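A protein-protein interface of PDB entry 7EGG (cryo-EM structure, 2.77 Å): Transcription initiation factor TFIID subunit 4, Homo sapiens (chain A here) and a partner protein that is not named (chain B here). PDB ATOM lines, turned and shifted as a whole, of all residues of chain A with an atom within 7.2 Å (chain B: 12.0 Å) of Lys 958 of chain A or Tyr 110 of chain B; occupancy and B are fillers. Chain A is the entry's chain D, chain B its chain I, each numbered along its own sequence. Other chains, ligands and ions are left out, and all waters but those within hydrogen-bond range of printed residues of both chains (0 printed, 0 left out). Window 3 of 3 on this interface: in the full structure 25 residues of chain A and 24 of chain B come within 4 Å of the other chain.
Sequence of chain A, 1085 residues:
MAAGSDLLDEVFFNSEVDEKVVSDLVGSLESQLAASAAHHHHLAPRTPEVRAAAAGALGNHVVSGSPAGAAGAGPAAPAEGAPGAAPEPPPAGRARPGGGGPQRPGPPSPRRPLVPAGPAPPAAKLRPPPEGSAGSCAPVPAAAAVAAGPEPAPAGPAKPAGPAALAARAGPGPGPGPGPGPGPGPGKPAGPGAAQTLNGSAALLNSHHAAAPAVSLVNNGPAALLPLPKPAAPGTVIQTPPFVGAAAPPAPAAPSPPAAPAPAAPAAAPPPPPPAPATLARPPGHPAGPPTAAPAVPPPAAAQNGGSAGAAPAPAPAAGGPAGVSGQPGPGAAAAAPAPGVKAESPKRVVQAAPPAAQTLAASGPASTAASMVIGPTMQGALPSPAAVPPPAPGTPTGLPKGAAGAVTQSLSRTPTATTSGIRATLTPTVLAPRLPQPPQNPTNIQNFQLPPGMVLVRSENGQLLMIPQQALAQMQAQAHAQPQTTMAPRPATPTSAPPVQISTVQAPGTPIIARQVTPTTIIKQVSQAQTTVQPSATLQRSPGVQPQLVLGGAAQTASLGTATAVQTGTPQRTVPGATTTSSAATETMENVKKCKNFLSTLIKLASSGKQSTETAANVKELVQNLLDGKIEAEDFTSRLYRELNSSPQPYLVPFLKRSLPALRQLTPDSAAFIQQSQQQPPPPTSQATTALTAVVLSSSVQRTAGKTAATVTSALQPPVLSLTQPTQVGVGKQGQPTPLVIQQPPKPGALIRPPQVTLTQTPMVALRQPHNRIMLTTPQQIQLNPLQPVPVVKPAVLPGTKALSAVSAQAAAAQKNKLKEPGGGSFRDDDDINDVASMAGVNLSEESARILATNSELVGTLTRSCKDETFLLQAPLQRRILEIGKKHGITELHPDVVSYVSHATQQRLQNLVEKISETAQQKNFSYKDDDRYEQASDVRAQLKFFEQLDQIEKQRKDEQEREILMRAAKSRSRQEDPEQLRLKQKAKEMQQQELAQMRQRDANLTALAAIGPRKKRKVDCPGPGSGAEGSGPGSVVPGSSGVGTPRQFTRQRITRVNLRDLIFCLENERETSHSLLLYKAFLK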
ATOM      1  N   GLU A 948      16.684  -2.992  13.530  1.00  0.00           N
ATOM      2  CA  GLU A 948      15.679  -4.065  13.304  1.00  0.00           C
ATOM      3  C   GLU A 948      14.621  -3.604  12.312  1.00  0.00           C
ATOM      4  O   GLU A 948      14.210  -4.423  11.503  1.00  0.00           O
ATOM      5  CB  GLU A 948      15.045  -4.518  14.617  1.00  0.00           C
ATOM      6  CG  GLU A 948      13.584  -4.170  14.787  1.00  0.00           C
ATOM      7  CD  GLU A 948      13.105  -4.290  16.221  1.00  0.00           C
ATOM      8  OE1 GLU A 948      13.922  -4.673  17.081  1.00  0.00           O
ATOM      9  OE2 GLU A 948      11.920  -3.993  16.476  1.00  0.00           O
ATOM     10  N   LEU A 950      15.089  -1.446   9.870  1.00  0.00           N
ATOM     11  CA  LEU A 950      15.736  -1.525   8.530  1.00  0.00           C
ATOM     12  C   LEU A 950      15.732  -2.970   8.031  1.00  0.00           C
ATOM     13  O   LEU A 950      15.460  -3.201   6.825  1.00  0.00           O
ATOM     14  CB  LEU A 950      17.174  -1.029   8.626  1.00  0.00           C
ATOM     15  CG  LEU A 950      17.368   0.421   9.040  1.00  0.00           C
ATOM     16  CD1 LEU A 950      18.843   0.777   8.976  1.00  0.00           C
ATOM     17  CD2 LEU A 950      16.562   1.337   8.143  1.00  0.00           C
ATOM     18  N   ASP A 951      15.998  -3.922   8.922  1.00  0.00           N
ATOM     19  CA  ASP A 951      15.927  -5.356   8.522  1.00  0.00           C
ATOM     20  C   ASP A 951      14.522  -5.768   8.112  1.00  0.00           C
ATOM     21  O   ASP A 951      14.415  -6.499   7.141  1.00  0.00           O
ATOM     22  CB  ASP A 951      16.487  -6.291   9.580  1.00  0.00           C
ATOM     23  CG  ASP A 951      17.923  -6.679   9.283  1.00  0.00           C
ATOM     24  OD1 ASP A 951      18.367  -6.425   8.149  1.00  0.00           O
ATOM     25  OD2 ASP A 951      18.582  -7.228  10.183  1.00  0.00           O
ATOM     26  N   GLN A 952      13.494  -5.307   8.805  1.00  0.00           N
ATOM     27  CA  GLN A 952      12.109  -5.608   8.380  1.00  0.00           C
ATOM     28  C   GLN A 952      11.837  -4.995   7.015  1.00  0.00           C
ATOM     29  O   GLN A 952      11.148  -5.634   6.242  1.00  0.00           O
ATOM     30  CB  GLN A 952      11.053  -5.291   9.433  1.00  0.00           C
ATOM     31  CG  GLN A 952      10.203  -4.073   9.107  1.00  0.00           C
ATOM     32  CD  GLN A 952       9.828  -3.272  10.329  1.00  0.00           C
ATOM     33  OE1 GLN A 952      10.054  -3.689  11.462  1.00  0.00           O
ATOM     34  NE2 GLN A 952       9.253  -2.102  10.107  1.00  0.00           N
ATOM     35  N   ILE A 953      12.349  -3.807   6.737  1.00  0.00           N
ATOM     36  CA  ILE A 953      12.180  -3.214   5.379  1.00  0.00           C
ATOM     37  C   ILE A 953      12.856  -4.113   4.349  1.00  0.00           C
ATOM     38  O   ILE A 953      12.166  -4.474   3.390  1.00  0.00           O
ATOM     39  CB  ILE A 953      12.684  -1.756   5.317  1.00  0.00           C
ATOM     40  CG1 ILE A 953      11.562  -0.742   5.541  1.00  0.00           C
ATOM     41  CG2 ILE A 953      13.421  -1.487   4.018  1.00  0.00           C
ATOM     42  CD1 ILE A 953      11.188  -0.542   6.987  1.00  0.00           C
ATOM     43  N   GLU A 954      14.068  -4.602   4.610  1.00  0.00           N
ATOM     44  CA  GLU A 954      14.695  -5.559   3.651  1.00  0.00           C
ATOM     45  C   GLU A 954      13.834  -6.808   3.492  1.00  0.00           C
ATOM     46  O   GLU A 954      13.679  -7.243   2.368  1.00  0.00           O
ATOM     47  CB  GLU A 954      16.033  -6.049   4.177  1.00  0.00           C
ATOM     48  CG  GLU A 954      16.869  -6.782   3.159  1.00  0.00           C
ATOM     49  CD  GLU A 954      18.327  -6.872   3.569  1.00  0.00           C
ATOM     50  OE1 GLU A 954      18.913  -7.957   3.421  1.00  0.00           O
ATOM     51  OE2 GLU A 954      18.870  -5.854   4.039  1.00  0.00           O
ATOM     52  N   LYS A 955      13.273  -7.338   4.578  1.00  0.00           N
ATOM     53  CA  LYS A 955      12.448  -8.563   4.507  1.00  0.00           C
ATOM     54  C   LYS A 955      11.204  -8.310   3.672  1.00  0.00           C
ATOM     55  O   LYS A 955      10.924  -9.152   2.831  1.00  0.00           O
ATOM     56  CB  LYS A 955      12.033  -9.045   5.886  1.00  0.00           C
ATOM     57  CG  LYS A 955      11.323 -10.388   5.930  1.00  0.00           C
ATOM     58  CD  LYS A 955      10.998 -10.810   7.348  1.00  0.00           C
ATOM     59  CE  LYS A 955      11.256 -12.279   7.611  1.00  0.00           C
ATOM     60  NZ  LYS A 955      11.689 -12.512   9.008  1.00  0.00           N
ATOM     61  N   GLN A 956      10.525  -7.177   3.837  1.00  0.00           N
ATOM     62  CA  GLN A 956       9.359  -6.885   2.977  1.00  0.00           C
ATOM     63  C   GLN A 956       9.813  -6.731   1.531  1.00  0.00           C
ATOM     64  O   GLN A 956       9.174  -7.332   0.675  1.00  0.00           O
ATOM     65  CB  GLN A 956       8.565  -5.686   3.463  1.00  0.00           C
ATOM     66  CG  GLN A 956       8.264  -5.693   4.953  1.00  0.00           C
ATOM     67  CD  GLN A 956       7.733  -7.015   5.448  1.00  0.00           C
ATOM     68  OE1 GLN A 956       7.781  -7.314   6.640  1.00  0.00           O
ATOM     69  NE2 GLN A 956       7.217  -7.817   4.531  1.00  0.00           N
ATOM     70  N   ARG A 957      10.927  -6.071   1.263  1.00  0.00           N
ATOM     71  CA  ARG A 957      11.327  -6.003  -0.165  1.00  0.00           C
ATOM     72  C   ARG A 957      11.533  -7.418  -0.684  1.00  0.00           C
ATOM     73  O   ARG A 957      10.957  -7.722  -1.716  1.00  0.00           O
ATOM     74  CB  ARG A 957      12.671  -5.309  -0.387  1.00  0.00           C
ATOM     75  CG  ARG A 957      12.547  -3.871  -0.861  1.00  0.00           C
ATOM     76  CD  ARG A 957      12.559  -2.859   0.264  1.00  0.00           C
ATOM     77  NE  ARG A 957      11.854  -1.652  -0.126  1.00  0.00           N
ATOM     78  CZ  ARG A 957      12.213  -0.427   0.231  1.00  0.00           C
ATOM     79  NH1 ARG A 957      13.288  -0.244   0.976  1.00  0.00           N
ATOM     80  NH2 ARG A 957      11.506   0.612  -0.171  1.00  0.00           N
ATOM     81  N   LYS A 958      12.227  -8.279   0.056  1.00  0.00           N
ATOM     82  CA  LYS A 958      12.531  -9.625  -0.482  1.00  0.00           C
ATOM     83  C   LYS A 958      11.217 -10.350  -0.730  1.00  0.00           C
ATOM     84  O   LYS A 958      11.042 -10.886  -1.822  1.00  0.00           O
ATOM     85  CB  LYS A 958      13.350 -10.432   0.523  1.00  0.00           C
ATOM     86  CG  LYS A 958      14.824 -10.073   0.567  1.00  0.00           C
ATOM     87  CD  LYS A 958      15.303  -9.508  -0.748  1.00  0.00           C
ATOM     88  CE  LYS A 958      16.636 -10.079  -1.175  1.00  0.00           C
ATOM     89  NZ  LYS A 958      16.550 -11.539  -1.408  1.00  0.00           N
ATOM     90  N   ASP A 959      10.297 -10.282   0.215  1.00  0.00           N
ATOM     91  CA  ASP A 959       9.052 -11.061   0.060  1.00  0.00           C
ATOM     92  C   ASP A 959       8.292 -10.551  -1.157  1.00  0.00           C
ATOM     93  O   ASP A 959       7.910 -11.368  -1.977  1.00  0.00           O
ATOM     94  CB  ASP A 959       8.249 -11.059   1.360  1.00  0.00           C
ATOM     95  CG  ASP A 959       8.754 -12.071   2.372  1.00  0.00           C
ATOM     96  OD1 ASP A 959       9.851 -11.854   2.921  1.00  0.00           O
ATOM     97  OD2 ASP A 959       8.052 -13.077   2.591  1.00  0.00           O
ATOM     98  N   GLU A 960       8.182  -9.237  -1.309  1.00  0.00           N
ATOM     99  CA  GLU A 960       7.426  -8.660  -2.446  1.00  0.00           C
ATOM    100  C   GLU A 960       8.106  -9.047  -3.768  1.00  0.00           C
ATOM    101  O   GLU A 960       7.386  -9.481  -4.684  1.00  0.00           O
ATOM    102  CB  GLU A 960       7.325  -7.150  -2.279  1.00  0.00           C
ATOM    103  CG  GLU A 960       6.159  -6.704  -1.411  1.00  0.00           C
ATOM    104  CD  GLU A 960       5.952  -7.442  -0.099  1.00  0.00           C
ATOM    105  OE1 GLU A 960       6.027  -8.684  -0.098  1.00  0.00           O
ATOM    106  OE2 GLU A 960       5.703  -6.771   0.922  1.00  0.00           O
ATOM    107  N   GLN A 961       9.439  -9.005  -3.837  1.00  0.00           N
ATOM    108  CA  GLN A 961      10.152  -9.414  -5.068  1.00  0.00           C
ATOM    109  C   GLN A 961       9.885 -10.885  -5.388  1.00  0.00           C
ATOM    110  O   GLN A 961       9.482 -11.165  -6.521  1.00  0.00           O
ATOM    111  CB  GLN A 961      11.654  -9.243  -4.876  1.00  0.00           C
ATOM    112  CG  GLN A 961      12.089  -7.786  -4.900  1.00  0.00           C
ATOM    113  CD  GLN A 961      13.585  -7.640  -4.801  1.00  0.00           C
ATOM    114  OE1 GLN A 961      14.329  -8.612  -4.901  1.00  0.00           O
ATOM    115  NE2 GLN A 961      14.038  -6.412  -4.609  1.00  0.00           N
ATOM    116  N   GLU A 962       9.973 -11.768  -4.397  1.00  0.00           N
ATOM    117  CA  GLU A 962       9.664 -13.194  -4.665  1.00  0.00           C
ATOM    118  C   GLU A 962       8.197 -13.345  -5.107  1.00  0.00           C
ATOM    119  O   GLU A 962       7.971 -14.045  -6.096  1.00  0.00           O
ATOM    120  CB  GLU A 962      10.115 -14.101  -3.520  1.00  0.00           C
ATOM    121  CG  GLU A 962       9.041 -14.400  -2.495  1.00  0.00           C
ATOM    122  CD  GLU A 962       9.505 -15.298  -1.362  1.00  0.00           C
ATOM    123  OE1 GLU A 962      10.731 -15.453  -1.200  1.00  0.00           O
ATOM    124  OE2 GLU A 962       8.640 -15.839  -0.649  1.00  0.00           O
ATOM    125  N   ARG A 963       7.243 -12.662  -4.476  1.00  0.00           N
ATOM    126  CA  ARG A 963       5.835 -12.874  -4.873  1.00  0.00           C
ATOM    127  C   ARG A 963       5.693 -12.427  -6.327  1.00  0.00           C
ATOM    128  O   ARG A 963       5.032 -13.140  -7.094  1.00  0.00           O
ATOM    129  CB  ARG A 963       4.895 -12.025  -4.015  1.00  0.00           C
ATOM    130  CG  ARG A 963       3.586 -11.660  -4.697  1.00  0.00           C
ATOM    131  CD  ARG A 963       2.743 -10.761  -3.818  1.00  0.00           C
ATOM    132  NE  ARG A 963       3.389  -9.496  -3.501  1.00  0.00           N
ATOM    133  CZ  ARG A 963       3.126  -8.345  -4.109  1.00  0.00           C
ATOM    134  NH1 ARG A 963       2.224  -8.297  -5.073  1.00  0.00           N
ATOM    135  NH2 ARG A 963       3.760  -7.246  -3.747  1.00  0.00           N
ATOM    136  N   GLU A 964       6.303 -11.300  -6.690  1.00  0.00           N
ATOM    137  CA  GLU A 964       6.150 -10.760  -8.061  1.00  0.00           C
ATOM    138  C   GLU A 964       6.794 -11.717  -9.065  1.00  0.00           C
ATOM    139  O   GLU A 964       6.172 -11.964 -10.115  1.00  0.00           O
ATOM    140  CB  GLU A 964       6.739  -9.356  -8.135  1.00  0.00           C
ATOM    141  CG  GLU A 964       7.080  -8.902  -9.543  1.00  0.00           C
ATOM    142  CD  GLU A 964       8.542  -9.054  -9.933  1.00  0.00           C
ATOM    143  OE1 GLU A 964       9.186 -10.001  -9.446  1.00  0.00           O
ATOM    144  OE2 GLU A 964       9.033  -8.218 -10.717  1.00  0.00           O
ATOM    145  N   ILE A 965       7.966 -12.273  -8.747  1.00  0.00           N
ATOM    146  CA  ILE A 965       8.570 -13.267  -9.683  1.00  0.00           C
ATOM    147  C   ILE A 965       7.692 -14.519  -9.792  1.00  0.00           C
ATOM    148  O   ILE A 965       7.590 -15.033 -10.899  1.00  0.00           O
ATOM    149  CB  ILE A 965      10.075 -13.547  -9.480  1.00  0.00           C
ATOM    150  CG1 ILE A 965      10.630 -14.432 -10.598  1.00  0.00           C
ATOM    151  CG2 ILE A 965      10.370 -14.145  -8.117  1.00  0.00           C
ATOM    152  CD1 ILE A 965      10.359 -15.906 -10.403  1.00  0.00           C
ATOM    153  N   LEU B 106      17.244 -23.097  15.322  1.00  0.00           N
ATOM    154  CA  LEU B 106      17.228 -22.416  14.039  1.00  0.00           C
ATOM    155  C   LEU B 106      17.235 -20.906  14.253  1.00  0.00           C
ATOM    156  O   LEU B 106      16.987 -20.405  15.351  1.00  0.00           O
ATOM    157  CB  LEU B 106      16.008 -22.830  13.211  1.00  0.00           C
ATOM    158  CG  LEU B 106      16.090 -24.052  12.285  1.00  0.00           C
ATOM    159  CD1 LEU B 106      17.132 -23.832  11.203  1.00  0.00           C
ATOM    160  CD2 LEU B 106      16.348 -25.358  13.024  1.00  0.00           C
ATOM    161  N   ILE B 107      17.529 -20.178  13.181  1.00  0.00           N
ATOM    162  CA  ILE B 107      17.705 -18.733  13.235  1.00  0.00           C
ATOM    163  C   ILE B 107      16.564 -18.076  12.474  1.00  0.00           C
ATOM    164  O   ILE B 107      16.239 -18.489  11.354  1.00  0.00           O
ATOM    165  CB  ILE B 107      19.067 -18.318  12.656  1.00  0.00           C
ATOM    166  CG1 ILE B 107      20.189 -18.987  13.432  1.00  0.00           C
ATOM    167  CG2 ILE B 107      19.264 -16.815  12.730  1.00  0.00           C
ATOM    168  CD1 ILE B 107      21.519 -18.747  12.828  1.00  0.00           C
ATOM    169  N   LYS B 108      15.957 -17.064  13.082  1.00  0.00           N
ATOM    170  CA  LYS B 108      14.990 -16.244  12.372  1.00  0.00           C
ATOM    171  C   LYS B 108      15.718 -15.399  11.329  1.00  0.00           C
ATOM    172  O   LYS B 108      16.793 -14.860  11.610  1.00  0.00           O
ATOM    173  CB  LYS B 108      14.226 -15.348  13.347  1.00  0.00           C
ATOM    174  CG  LYS B 108      12.898 -15.918  13.849  1.00  0.00           C
ATOM    175  CD  LYS B 108      13.089 -17.143  14.737  1.00  0.00           C
ATOM    176  CE  LYS B 108      13.909 -16.812  15.975  1.00  0.00           C
ATOM    177  NZ  LYS B 108      14.151 -18.018  16.814  1.00  0.00           N
ATOM    178  N   PRO B 109      15.164 -15.267  10.121  1.00  0.00           N
ATOM    179  CA  PRO B 109      15.954 -14.736   9.002  1.00  0.00           C
ATOM    180  C   PRO B 109      16.210 -13.236   9.040  1.00  0.00           C
ATOM    181  O   PRO B 109      17.268 -12.785   8.592  1.00  0.00           O
ATOM    182  CB  PRO B 109      15.116 -15.121   7.776  1.00  0.00           C
ATOM    183  CG  PRO B 109      13.732 -15.232   8.289  1.00  0.00           C
ATOM    184  CD  PRO B 109      13.841 -15.747   9.688  1.00  0.00           C
ATOM    185  N   TYR B 110      15.272 -12.447   9.552  1.00  0.00           N
ATOM    186  CA  TYR B 110      15.414 -10.993   9.572  1.00  0.00           C
ATOM    187  C   TYR B 110      15.010 -10.435  10.928  1.00  0.00           C
ATOM    188  O   TYR B 110      14.222  -9.493  11.036  1.00  0.00           O
ATOM    189  CB  TYR B 110      14.606 -10.351   8.450  1.00  0.00           C
ATOM    190  CG  TYR B 110      15.273 -10.454   7.101  1.00  0.00           C
ATOM    191  CD1 TYR B 110      16.372  -9.665   6.790  1.00  0.00           C
ATOM    192  CD2 TYR B 110      14.812 -11.347   6.143  1.00  0.00           C
ATOM    193  CE1 TYR B 110      16.990  -9.757   5.558  1.00  0.00           C
ATOM    194  CE2 TYR B 110      15.423 -11.447   4.909  1.00  0.00           C
ATOM    195  CZ  TYR B 110      16.512 -10.649   4.623  1.00  0.00           C
ATOM    196  OH  TYR B 110      17.125 -10.744   3.395  1.00  0.00           O
ATOM    197  N   SER B 111      15.552 -11.028  11.993  1.00  0.00           N
ATOM    198  CA  SER B 111      15.228 -10.573  13.340  1.00  0.00           C
ATOM    199  C   SER B 111      15.903  -9.249  13.672  1.00  0.00           C
ATOM    200  O   SER B 111      15.415  -8.505  14.530  1.00  0.00           O
ATOM    201  CB  SER B 111      15.625 -11.639  14.357  1.00  0.00           C
ATOM    202  OG  SER B 111      16.909 -12.159  14.065  1.00  0.00           O
ATOM    203  N   GLY B 112      17.018  -8.939  13.016  1.00  0.00           N
ATOM    204  CA  GLY B 112      17.716  -7.700  13.255  1.00  0.00           C
ATOM    205  C   GLY B 112      19.090  -7.927  13.851  1.00  0.00           C
ATOM    206  O   GLY B 112      19.797  -8.874  13.496  1.00  0.00           O
ATOM    207  N   PRO B 113      19.506  -7.041  14.755  1.00  0.00           N
ATOM    208  CA  PRO B 113      20.707  -7.316  15.553  1.00  0.00           C
ATOM    209  C   PRO B 113      20.461  -8.442  16.542  1.00  0.00           C
ATOM    210  O   PRO B 113      19.679  -8.289  17.485  1.00  0.00           O
ATOM    211  CB  PRO B 113      20.975  -5.982  16.263  1.00  0.00           C
ATOM    212  CG  PRO B 113      19.687  -5.243  16.206  1.00  0.00           C
ATOM    213  CD  PRO B 113      19.013  -5.668  14.948  1.00  0.00           C
ATOM    214  N   ARG B 114      21.113  -9.582  16.327  1.00  0.00           N
ATOM    215  CA  ARG B 114      20.863 -10.777  17.127  1.00  0.00           C
ATOM    216  C   ARG B 114      21.487 -10.613  18.504  1.00  0.00           C
ATOM    217  O   ARG B 114      22.713 -10.619  18.643  1.00  0.00           O
ATOM    218  CB  ARG B 114      21.417 -12.006  16.418  1.00  0.00           C
ATOM    219  CG  ARG B 114      20.508 -12.562  15.346  1.00  0.00           C
ATOM    220  CD  ARG B 114      21.317 -13.078  14.181  1.00  0.00           C
ATOM    221  NE  ARG B 114      20.483 -13.387  13.027  1.00  0.00           N
ATOM    222  CZ  ARG B 114      20.938 -13.442  11.781  1.00  0.00           C
ATOM    223  NH1 ARG B 114      22.219 -13.211  11.535  1.00  0.00           N
ATOM    224  NH2 ARG B 114      20.113 -13.728  10.783  1.00  0.00           N
ATOM    225  N   LEU B 115      20.644 -10.483  19.519  1.00  0.00           N
ATOM    226  CA  LEU B 115      21.061 -10.210  20.884  1.00  0.00           C
ATOM    227  C   LEU B 115      20.252 -11.082  21.831  1.00  0.00           C
ATOM    228  O   LEU B 115      19.189 -11.587  21.460  1.00  0.00           O
ATOM    229  CB  LEU B 115      20.869  -8.728  21.235  1.00  0.00           C
ATOM    230  CG  LEU B 115      21.924  -7.728  20.765  1.00  0.00           C
ATOM    231  CD1 LEU B 115      21.782  -6.459  21.560  1.00  0.00           C
ATOM    232  CD2 LEU B 115      23.326  -8.282  20.909  1.00  0.00           C
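Among the printed residues, merely in contact across the chains: Glu 948 of chain A with Pro 113 of chain B (3.8 Å), Asp 951 of chain A with Tyr 110 of chain B (3.7 Å), Asp 951 of chain A with Gly 112 of chain B (3.2 Å), Lys 955 of chain A with Pro 109 of chain B (3.5 Å), Lys 955 of chain A with Tyr 110 of chain B (3.6 Å) and Lys 958 of chain A with Tyr 110 of chain B (3.7 Å).
Along chain A the printed residues that touch a printed residue of chain B span positions 948 to 958.
The side-chain carboxylate (OE1) of Glu 954 of chain A sits at hydrogen-bond distance from the side-chain hydroxyl (OH) of Tyr 110 of chain B (3.3 Å).
Printed residues of chain B within 4 Å of Glu 948 of chain A: Pro 113 (3.8 Å). Printed residues of chain B within 4 Å of Asp 951 of chain A: Tyr 110 (3.7 Å) and Gly 112 (3.2 Å). Glu 954 of chain A touches just one residue of chain B: Tyr 110 (3.3 Å). Of chain B, only Pro 109 and Tyr 110 come within 4 Å of Lys 955 of chain A. No residue of chain B comes within 4 Å of Gln 956 of chain A. Lys 958 of chain A touches one residue of chain B. No residue of chain B comes within 4 Å of Glu 960 of chain A. No residue of chain B comes within 4 Å of Glu 962 of chain A. Arg 963 of chain A touches none of the printed residues of chain B. Of the printed residues of chain A, Pro 109 of chain B touches Lys 955 (3.5 Å). Of chain A, only Asp 951, Glu 954, Lys 955 and Lys 958 come within 4 Å of Tyr 110 of chain B. Of the printed residues of chain A, Gly 112 of chain B touches Asp 951. Printed residues of chain A within 4 Å of Pro 113 of chain B: Glu 948. The nearest residue of chain B that does not touch Lys 958 of chain A is Pro 109 of chain B (8.8 Å). The nearest printed residue of chain A that does not touch Pro 113 of chain B is Asp 951 of chain A (4.7 Å).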
